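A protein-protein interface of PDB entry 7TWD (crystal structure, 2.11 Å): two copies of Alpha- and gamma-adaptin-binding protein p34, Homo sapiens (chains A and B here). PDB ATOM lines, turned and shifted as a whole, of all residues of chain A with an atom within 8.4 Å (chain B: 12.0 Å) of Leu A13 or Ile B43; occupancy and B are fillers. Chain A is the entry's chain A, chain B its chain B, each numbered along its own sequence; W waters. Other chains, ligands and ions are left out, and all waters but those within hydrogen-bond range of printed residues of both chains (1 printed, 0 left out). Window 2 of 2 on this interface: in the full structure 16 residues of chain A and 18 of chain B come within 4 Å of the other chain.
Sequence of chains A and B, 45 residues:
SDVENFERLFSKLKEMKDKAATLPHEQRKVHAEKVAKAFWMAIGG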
ATOM      1  N   PHE A   6      38.013  -0.953 -39.909  1.00  0.00           N
ATOM      2  CA  PHE A   6      37.208  -0.172 -38.976  1.00  0.00           C
ATOM      3  C   PHE A   6      35.728  -0.276 -39.316  1.00  0.00           C
ATOM      4  O   PHE A   6      34.888  -0.431 -38.422  1.00  0.00           O
ATOM      5  CB  PHE A   6      37.669   1.287 -38.990  1.00  0.00           C
ATOM      6  CG  PHE A   6      36.736   2.232 -38.285  1.00  0.00           C
ATOM      7  CD1 PHE A   6      36.821   2.414 -36.914  1.00  0.00           C
ATOM      8  CD2 PHE A   6      35.785   2.949 -38.994  1.00  0.00           C
ATOM      9  CE1 PHE A   6      35.969   3.286 -36.262  1.00  0.00           C
ATOM     10  CE2 PHE A   6      34.929   3.820 -38.348  1.00  0.00           C
ATOM     11  CZ  PHE A   6      35.021   3.990 -36.981  1.00  0.00           C
ATOM     12  N   GLU A   7      35.393  -0.197 -40.605  1.00  0.00           N
ATOM     13  CA  GLU A   7      34.008  -0.356 -41.040  1.00  0.00           C
ATOM     14  C   GLU A   7      33.435  -1.686 -40.569  1.00  0.00           C
ATOM     15  O   GLU A   7      32.324  -1.745 -40.026  1.00  0.00           O
ATOM     16  CB  GLU A   7      33.937  -0.254 -42.563  1.00  0.00           C
ATOM     17  CG  GLU A   7      32.668   0.363 -43.116  1.00  0.00           C
ATOM     18  CD  GLU A   7      32.929   1.158 -44.381  1.00  0.00           C
ATOM     19  OE1 GLU A   7      33.841   2.011 -44.373  1.00  0.00           O
ATOM     20  OE2 GLU A   7      32.238   0.913 -45.392  1.00  0.00           O
ATOM     21  N   ARG A   8      34.191  -2.769 -40.763  1.00  0.00           N
ATOM     22  CA  ARG A   8      33.725  -4.095 -40.372  1.00  0.00           C
ATOM     23  C   ARG A   8      33.576  -4.206 -38.860  1.00  0.00           C
ATOM     24  O   ARG A   8      32.552  -4.685 -38.356  1.00  0.00           O
ATOM     25  CB  ARG A   8      34.696  -5.151 -40.898  1.00  0.00           C
ATOM     26  CG  ARG A   8      34.170  -6.575 -40.883  1.00  0.00           C
ATOM     27  CD  ARG A   8      35.290  -7.540 -41.229  1.00  0.00           C
ATOM     28  NE  ARG A   8      36.440  -7.349 -40.350  1.00  0.00           N
ATOM     29  CZ  ARG A   8      37.094  -8.336 -39.746  1.00  0.00           C
ATOM     30  NH1 ARG A   8      36.725  -9.594 -39.939  1.00  0.00           N
ATOM     31  NH2 ARG A   8      38.128  -8.065 -38.961  1.00  0.00           N
ATOM     32  N   LEU A   9      34.591  -3.762 -38.117  1.00  0.00           N
ATOM     33  CA  LEU A   9      34.577  -3.921 -36.667  1.00  0.00           C
ATOM     34  C   LEU A   9      33.560  -2.994 -36.012  1.00  0.00           C
ATOM     35  O   LEU A   9      32.953  -3.352 -34.996  1.00  0.00           O
ATOM     36  CB  LEU A   9      35.973  -3.671 -36.105  1.00  0.00           C
ATOM     37  CG  LEU A   9      36.881  -4.899 -36.071  1.00  0.00           C
ATOM     38  CD1 LEU A   9      38.287  -4.509 -35.654  1.00  0.00           C
ATOM     39  CD2 LEU A   9      36.305  -5.959 -35.145  1.00  0.00           C
ATOM     40  N   PHE A  10      33.370  -1.795 -36.571  1.00  0.00           N
ATOM     41  CA  PHE A  10      32.348  -0.894 -36.047  1.00  0.00           C
ATOM     42  C   PHE A  10      30.966  -1.526 -36.139  1.00  0.00           C
ATOM     43  O   PHE A  10      30.173  -1.445 -35.194  1.00  0.00           O
ATOM     44  CB  PHE A  10      32.383   0.437 -36.801  1.00  0.00           C
ATOM     45  CG  PHE A  10      31.470   1.490 -36.228  1.00  0.00           C
ATOM     46  CD1 PHE A  10      30.137   1.549 -36.600  1.00  0.00           C
ATOM     47  CD2 PHE A  10      31.951   2.425 -35.326  1.00  0.00           C
ATOM     48  CE1 PHE A  10      29.298   2.515 -36.078  1.00  0.00           C
ATOM     49  CE2 PHE A  10      31.117   3.395 -34.802  1.00  0.00           C
ATOM     50  CZ  PHE A  10      29.788   3.440 -35.178  1.00  0.00           C
ATOM     51  N   SER A  11      30.660  -2.161 -37.272  1.00  0.00           N
ATOM     52  CA  SER A  11      29.359  -2.801 -37.431  1.00  0.00           C
ATOM     53  C   SER A  11      29.244  -4.058 -36.580  1.00  0.00           C
ATOM     54  O   SER A  11      28.141  -4.411 -36.149  1.00  0.00           O
ATOM     55  CB  SER A  11      29.111  -3.126 -38.904  1.00  0.00           C
ATOM     56  OG  SER A  11      30.197  -3.850 -39.456  1.00  0.00           O
ATOM     57  N   LYS A  12      30.360  -4.745 -36.330  1.00  0.00           N
ATOM     58  CA  LYS A  12      30.322  -5.902 -35.442  1.00  0.00           C
ATOM     59  C   LYS A  12      30.119  -5.473 -33.995  1.00  0.00           C
ATOM     60  O   LYS A  12      29.453  -6.170 -33.221  1.00  0.00           O
ATOM     61  CB  LYS A  12      31.602  -6.722 -35.591  1.00  0.00           C
ATOM     62  CG  LYS A  12      31.650  -7.540 -36.869  1.00  0.00           C
ATOM     63  CD  LYS A  12      32.947  -8.317 -36.995  1.00  0.00           C
ATOM     64  CE  LYS A  12      32.865  -9.325 -38.129  1.00  0.00           C
ATOM     65  NZ  LYS A  12      34.201  -9.866 -38.490  1.00  0.00           N
ATOM     66  N   LEU A  13      30.688  -4.326 -33.613  1.00  0.00           N
ATOM     67  CA  LEU A  13      30.407  -3.767 -32.295  1.00  0.00           C
ATOM     68  C   LEU A  13      28.952  -3.335 -32.185  1.00  0.00           C
ATOM     69  O   LEU A  13      28.309  -3.550 -31.151  1.00  0.00           O
ATOM     70  CB  LEU A  13      31.339  -2.588 -32.017  1.00  0.00           C
ATOM     71  CG  LEU A  13      32.757  -2.917 -31.549  1.00  0.00           C
ATOM     72  CD1 LEU A  13      33.637  -1.681 -31.621  1.00  0.00           C
ATOM     73  CD2 LEU A  13      32.738  -3.482 -30.139  1.00  0.00           C
ATOM     74  N   LYS A  14      28.417  -2.722 -33.244  1.00  0.00           N
ATOM     75  CA  LYS A  14      27.016  -2.315 -33.243  1.00  0.00           C
ATOM     76  C   LYS A  14      26.093  -3.526 -33.187  1.00  0.00           C
ATOM     77  O   LYS A  14      25.101  -3.527 -32.449  1.00  0.00           O
ATOM     78  CB  LYS A  14      26.720  -1.467 -34.480  1.00  0.00           C
ATOM     79  CG  LYS A  14      25.254  -1.112 -34.663  1.00  0.00           C
ATOM     80  CD  LYS A  14      24.741  -0.258 -33.517  1.00  0.00           C
ATOM     81  CE  LYS A  14      23.614   0.655 -33.972  1.00  0.00           C
ATOM     82  NZ  LYS A  14      22.653  -0.052 -34.865  1.00  0.00           N
ATOM     83  N   GLU A  15      26.406  -4.566 -33.962  1.00  0.00           N
ATOM     84  CA  GLU A  15      25.611  -5.790 -33.927  1.00  0.00           C
ATOM     85  C   GLU A  15      25.655  -6.437 -32.548  1.00  0.00           C
ATOM     86  O   GLU A  15      24.631  -6.908 -32.040  1.00  0.00           O
ATOM     87  CB  GLU A  15      26.115  -6.760 -34.996  1.00  0.00           C
ATOM     88  CG  GLU A  15      25.519  -8.152 -34.925  1.00  0.00           C
ATOM     89  CD  GLU A  15      26.165  -9.103 -35.913  1.00  0.00           C
ATOM     90  OE1 GLU A  15      27.269  -9.605 -35.617  1.00  0.00           O
ATOM     91  OE2 GLU A  15      25.571  -9.343 -36.985  1.00  0.00           O
ATOM     92  N   MET A  16      26.836  -6.465 -31.926  1.00  0.00           N
ATOM     93  CA  MET A  16      26.960  -7.023 -30.584  1.00  0.00           C
ATOM     94  C   MET A  16      26.217  -6.170 -29.563  1.00  0.00           C
ATOM     95  O   MET A  16      25.579  -6.702 -28.646  1.00  0.00           O
ATOM     96  CB  MET A  16      28.439  -7.149 -30.220  1.00  0.00           C
ATOM     97  CG  MET A  16      28.720  -7.650 -28.816  1.00  0.00           C
ATOM     98  SD  MET A  16      30.482  -7.549 -28.443  1.00  0.00           S
ATOM     99  CE  MET A  16      31.150  -8.545 -29.772  1.00  0.00           C
ATOM    100  N   LYS A  17      26.289  -4.844 -29.710  1.00  0.00           N
ATOM    101  CA  LYS A  17      25.513  -3.945 -28.860  1.00  0.00           C
ATOM    102  C   LYS A  17      24.018  -4.191 -29.014  1.00  0.00           C
ATOM    103  O   LYS A  17      23.280  -4.226 -28.021  1.00  0.00           O
ATOM    104  CB  LYS A  17      25.858  -2.495 -29.202  1.00  0.00           C
ATOM    105  CG  LYS A  17      25.006  -1.426 -28.526  1.00  0.00           C
ATOM    106  CD  LYS A  17      24.987  -1.539 -27.014  1.00  0.00           C
ATOM    107  CE  LYS A  17      24.188  -0.392 -26.412  1.00  0.00           C
ATOM    108  NZ  LYS A  17      23.812  -0.627 -24.993  1.00  0.00           N
ATOM    109  N   ASP A  18      23.554  -4.372 -30.253  1.00  0.00           N
ATOM    110  CA  ASP A  18      22.127  -4.552 -30.494  1.00  0.00           C
ATOM    111  C   ASP A  18      21.634  -5.887 -29.949  1.00  0.00           C
ATOM    112  O   ASP A  18      20.548  -5.958 -29.359  1.00  0.00           O
ATOM    113  CB  ASP A  18      21.835  -4.437 -31.990  1.00  0.00           C
ATOM    114  CG  ASP A  18      22.004  -3.021 -32.508  1.00  0.00           C
ATOM    115  OD1 ASP A  18      21.961  -2.077 -31.691  1.00  0.00           O
ATOM    116  OD2 ASP A  18      22.186  -2.852 -33.733  1.00  0.00           O
ATOM    117  N   LYS A  19      22.411  -6.955 -30.139  1.00  0.00           N
ATOM    118  CA  LYS A  19      22.050  -8.247 -29.563  1.00  0.00           C
ATOM    119  C   LYS A  19      21.960  -8.157 -28.045  1.00  0.00           C
ATOM    120  O   LYS A  19      20.993  -8.630 -27.438  1.00  0.00           O
ATOM    121  CB  LYS A  19      23.071  -9.311 -29.967  1.00  0.00           C
ATOM    122  CG  LYS A  19      23.028  -9.742 -31.419  1.00  0.00           C
ATOM    123  CD  LYS A  19      24.217 -10.643 -31.716  1.00  0.00           C
ATOM    124  CE  LYS A  19      24.036 -11.436 -32.994  1.00  0.00           C
ATOM    125  NZ  LYS A  19      25.193 -12.349 -33.219  1.00  0.00           N
ATOM    126  N   ALA A  20      22.967  -7.545 -27.417  1.00  0.00           N
ATOM    127  CA  ALA A  20      22.980  -7.429 -25.962  1.00  0.00           C
ATOM    128  C   ALA A  20      21.795  -6.614 -25.459  1.00  0.00           C
ATOM    129  O   ALA A  20      21.221  -6.922 -24.409  1.00  0.00           O
ATOM    130  CB  ALA A  20      24.295  -6.803 -25.500  1.00  0.00           C
ATOM    131  N   ALA B  32      22.557 -16.697 -28.398  1.00  0.00           N
ATOM    132  CA  ALA B  32      23.496 -15.845 -29.120  1.00  0.00           C
ATOM    133  C   ALA B  32      23.563 -14.451 -28.506  1.00  0.00           C
ATOM    134  O   ALA B  32      24.635 -13.838 -28.453  1.00  0.00           O
ATOM    135  CB  ALA B  32      23.104 -15.766 -30.595  1.00  0.00           C
ATOM    136  N   GLU B  33      22.425 -13.938 -28.031  1.00  0.00           N
ATOM    137  CA  GLU B  33      22.409 -12.619 -27.410  1.00  0.00           C
ATOM    138  C   GLU B  33      23.055 -12.638 -26.030  1.00  0.00           C
ATOM    139  O   GLU B  33      23.666 -11.645 -25.619  1.00  0.00           O
ATOM    140  CB  GLU B  33      20.975 -12.099 -27.324  1.00  0.00           C
ATOM    141  CG  GLU B  33      20.409 -11.636 -28.659  1.00  0.00           C
ATOM    142  CD  GLU B  33      18.894 -11.567 -28.659  1.00  0.00           C
ATOM    143  OE1 GLU B  33      18.285 -11.863 -27.610  1.00  0.00           O
ATOM    144  OE2 GLU B  33      18.312 -11.214 -29.707  1.00  0.00           O
ATOM    145  N   LYS B  34      22.926 -13.750 -25.300  1.00  0.00           N
ATOM    146  CA  LYS B  34      23.639 -13.886 -24.033  1.00  0.00           C
ATOM    147  C   LYS B  34      25.146 -13.896 -24.255  1.00  0.00           C
ATOM    148  O   LYS B  34      25.897 -13.270 -23.498  1.00  0.00           O
ATOM    149  CB  LYS B  34      23.201 -15.162 -23.315  1.00  0.00           C
ATOM    150  CG  LYS B  34      21.812 -15.099 -22.704  1.00  0.00           C
ATOM    151  CD  LYS B  34      21.446 -16.436 -22.083  1.00  0.00           C
ATOM    152  CE  LYS B  34      20.077 -16.392 -21.427  1.00  0.00           C
ATOM    153  NZ  LYS B  34      19.672 -17.729 -20.914  1.00  0.00           N
ATOM    154  N   VAL B  35      25.603 -14.608 -25.288  1.00  0.00           N
ATOM    155  CA  VAL B  35      27.022 -14.601 -25.633  1.00  0.00           C
ATOM    156  C   VAL B  35      27.472 -13.186 -25.974  1.00  0.00           C
ATOM    157  O   VAL B  35      28.521 -12.720 -25.515  1.00  0.00           O
ATOM    158  CB  VAL B  35      27.292 -15.579 -26.791  1.00  0.00           C
ATOM    159  CG1 VAL B  35      28.620 -15.260 -27.468  1.00  0.00           C
ATOM    160  CG2 VAL B  35      27.274 -17.014 -26.287  1.00  0.00           C
ATOM    161  N   ALA B  36      26.670 -12.474 -26.772  1.00  0.00           N
ATOM    162  CA  ALA B  36      27.018 -11.108 -27.149  1.00  0.00           C
ATOM    163  C   ALA B  36      27.114 -10.202 -25.928  1.00  0.00           C
ATOM    164  O   ALA B  36      28.030  -9.375 -25.833  1.00  0.00           O
ATOM    165  CB  ALA B  36      25.995 -10.557 -28.142  1.00  0.00           C
ATOM    166  N   LYS B  37      26.181 -10.343 -24.984  1.00  0.00           N
ATOM    167  CA  LYS B  37      26.222  -9.512 -23.785  1.00  0.00           C
ATOM    168  C   LYS B  37      27.459  -9.808 -22.950  1.00  0.00           C
ATOM    169  O   LYS B  37      28.072  -8.892 -22.391  1.00  0.00           O
ATOM    170  CB  LYS B  37      24.956  -9.710 -22.951  1.00  0.00           C
ATOM    171  CG  LYS B  37      24.920  -8.838 -21.704  1.00  0.00           C
ATOM    172  CD  LYS B  37      23.524  -8.724 -21.124  1.00  0.00           C
ATOM    173  CE  LYS B  37      23.492  -7.689 -20.009  1.00  0.00           C
ATOM    174  NZ  LYS B  37      23.890  -6.341 -20.497  1.00  0.00           N
ATOM    175  N   ALA B  38      27.848 -11.082 -22.856  1.00  0.00           N
ATOM    176  CA  ALA B  38      29.054 -11.430 -22.111  1.00  0.00           C
ATOM    177  C   ALA B  38      30.286 -10.783 -22.733  1.00  0.00           C
ATOM    178  O   ALA B  38      31.126 -10.214 -22.028  1.00  0.00           O
ATOM    179  CB  ALA B  38      29.210 -12.950 -22.047  1.00  0.00           C
ATOM    180  N   PHE B  39      30.405 -10.857 -24.061  1.00  0.00           N
ATOM    181  CA  PHE B  39      31.521 -10.205 -24.741  1.00  0.00           C
ATOM    182  C   PHE B  39      31.447  -8.692 -24.592  1.00  0.00           C
ATOM    183  O   PHE B  39      32.471  -8.028 -24.392  1.00  0.00           O
ATOM    184  CB  PHE B  39      31.535 -10.589 -26.221  1.00  0.00           C
ATOM    185  CG  PHE B  39      32.168 -11.919 -26.500  1.00  0.00           C
ATOM    186  CD1 PHE B  39      33.543 -12.035 -26.618  1.00  0.00           C
ATOM    187  CD2 PHE B  39      31.390 -13.053 -26.655  1.00  0.00           C
ATOM    188  CE1 PHE B  39      34.128 -13.259 -26.879  1.00  0.00           C
ATOM    189  CE2 PHE B  39      31.972 -14.279 -26.917  1.00  0.00           C
ATOM    190  CZ  PHE B  39      33.340 -14.382 -27.028  1.00  0.00           C
ATOM    191  N   TRP B  40      30.240  -8.131 -24.691  1.00  0.00           N
ATOM    192  CA  TRP B  40      30.075  -6.686 -24.573  1.00  0.00           C
ATOM    193  C   TRP B  40      30.540  -6.184 -23.213  1.00  0.00           C
ATOM    194  O   TRP B  40      31.202  -5.145 -23.119  1.00  0.00           O
ATOM    195  CB  TRP B  40      28.613  -6.310 -24.815  1.00  0.00           C
ATOM    196  CG  TRP B  40      28.337  -4.847 -24.702  1.00  0.00           C
ATOM    197  CD1 TRP B  40      27.787  -4.195 -23.635  1.00  0.00           C
ATOM    198  CD2 TRP B  40      28.592  -3.847 -25.694  1.00  0.00           C
ATOM    199  NE1 TRP B  40      27.686  -2.852 -23.902  1.00  0.00           N
ATOM    200  CE2 TRP B  40      28.172  -2.611 -25.160  1.00  0.00           C
ATOM    201  CE3 TRP B  40      29.133  -3.874 -26.983  1.00  0.00           C
ATOM    202  CZ2 TRP B  40      28.279  -1.416 -25.868  1.00  0.00           C
ATOM    203  CZ3 TRP B  40      29.238  -2.688 -27.686  1.00  0.00           C
ATOM    204  CH2 TRP B  40      28.810  -1.476 -27.128  1.00  0.00           C
ATOM    205  N   MET B  41      30.206  -6.912 -22.143  1.00  0.00           N
ATOM    206  CA  MET B  41      30.660  -6.514 -20.816  1.00  0.00           C
ATOM    207  C   MET B  41      32.157  -6.741 -20.650  1.00  0.00           C
ATOM    208  O   MET B  41      32.835  -5.972 -19.958  1.00  0.00           O
ATOM    209  CB  MET B  41      29.889  -7.277 -19.739  1.00  0.00           C
ATOM    210  CG  MET B  41      28.381  -7.202 -19.867  1.00  0.00           C
ATOM    211  SD  MET B  41      27.717  -5.764 -19.017  1.00  0.00           S
ATOM    212  CE  MET B  41      28.304  -6.084 -17.359  1.00  0.00           C
ATOM    213  N   ALA B  42      32.690  -7.792 -21.279  1.00  0.00           N
ATOM    214  CA  ALA B  42      34.094  -8.143 -21.088  1.00  0.00           C
ATOM    215  C   ALA B  42      35.022  -7.066 -21.636  1.00  0.00           C
ATOM    216  O   ALA B  42      36.084  -6.802 -21.061  1.00  0.00           O
ATOM    217  CB  ALA B  42      34.393  -9.487 -21.751  1.00  0.00           C
ATOM    218  N   ILE B  43      34.642  -6.434 -22.745  1.00  0.00           N
ATOM    219  CA  ILE B  43      35.506  -5.455 -23.396  1.00  0.00           C
ATOM    220  C   ILE B  43      35.226  -4.065 -22.842  1.00  0.00           C
ATOM    221  O   ILE B  43      35.772  -3.068 -23.329  1.00  0.00           O
ATOM    222  CB  ILE B  43      35.332  -5.487 -24.926  1.00  0.00           C
ATOM    223  CG1 ILE B  43      33.942  -4.986 -25.316  1.00  0.00           C
ATOM    224  CG2 ILE B  43      35.565  -6.896 -25.454  1.00  0.00           C
ATOM    225  CD1 ILE B  43      33.696  -4.969 -26.811  1.00  0.00           C
ATOM    226  N   GLY B  44      34.382  -3.988 -21.819  1.00  0.00           N
ATOM    227  CA  GLY B  44      34.102  -2.727 -21.165  1.00  0.00           C
ATOM    228  C   GLY B  44      33.001  -1.902 -21.785  1.00  0.00           C
ATOM    229  O   GLY B  44      32.956  -0.688 -21.555  1.00  0.00           O
ATOM    230  N   GLY B  45      32.113  -2.512 -22.563  1.00  0.00           N
ATOM    231  CA  GLY B  45      31.020  -1.784 -23.178  1.00  0.00           C
ATOM    232  C   GLY B  45      30.047  -1.219 -22.161  1.00  0.00           C
ATOM    233  O   GLY B  45      29.722  -1.872 -21.168  1.00  0.00           O
ATOM    234  OXT GLY B  45      29.561  -0.097 -22.299  1.00  0.00           O
HETATM  235  O   HOH W   1      20.937  -6.701 -21.771  1.00  0.00           O
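O of Trp B40 lies within hydrogen-bond range of N of Gly B45, 2.8 Å away.
Among the printed residues, merely in contact across the chains: Leu A13 with Trp B40, Leu A13 with Ile B43, Met A16 with Ala B36, Met A16 with Phe B39, Met A16 with Trp B40, Lys A17 with Trp B40, Lys A19 with Glu B33, Lys A19 with Ala B36 and Ala A20 with Lys B37.
Leu A13 touches just these residues of chain B: Trp B40 (3.7 Å) and Ile B43 (3.8 Å). Ile B43 touches just one residue of chain A: Leu A13 (3.8 Å). No residue of chain B comes within 4 Å of Leu A9. Phe A10 touches none of the printed residues of chain B. No residue of chain B comes within 4 Å of Ser A11. No residue of chain B comes within 4 Å of Lys A14. Met A16 touches just these residues of chain B: Ala B36, Phe B39 and Trp B40. No residue of chain A comes within 4 Å of Ala B42. No residue of chain A comes within 4 Å of Gly B44. Printed residues of chain A within 4 Å of Lys B37: Ala A20. Of the printed residues of chain A, Ala B36 touches Met A16 (3.5 Å) and Lys A19 (3.7 Å). Val B35 touches none of the printed residues of chain A. Ala B32 touches none of the printed residues of chain A. The nearest residue of chain B that does not touch Leu A13 is Phe B39 (7.3 Å).
Of the 15 printed residues of chain A, 5 touch a printed residue of chain B. Along chain A the printed residues that touch a printed residue of chain B span positions 13 to 20. Hydrophobic or aromatic side chains of chain B that line the printed part of chain A: Ala B36, Phe B39, Trp B40 and Ile B43. Among the printed residues, 9 pairs touch across the chains. Among the printed residues, no Asp or Glu carboxylate lies within 4 Å of a Lys or Arg side-chain nitrogen of the other chain.
No position is printed for both chains.
Water W1 lies within hydrogen-bond range of O of Ala A20 and NZ of Lys B37.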
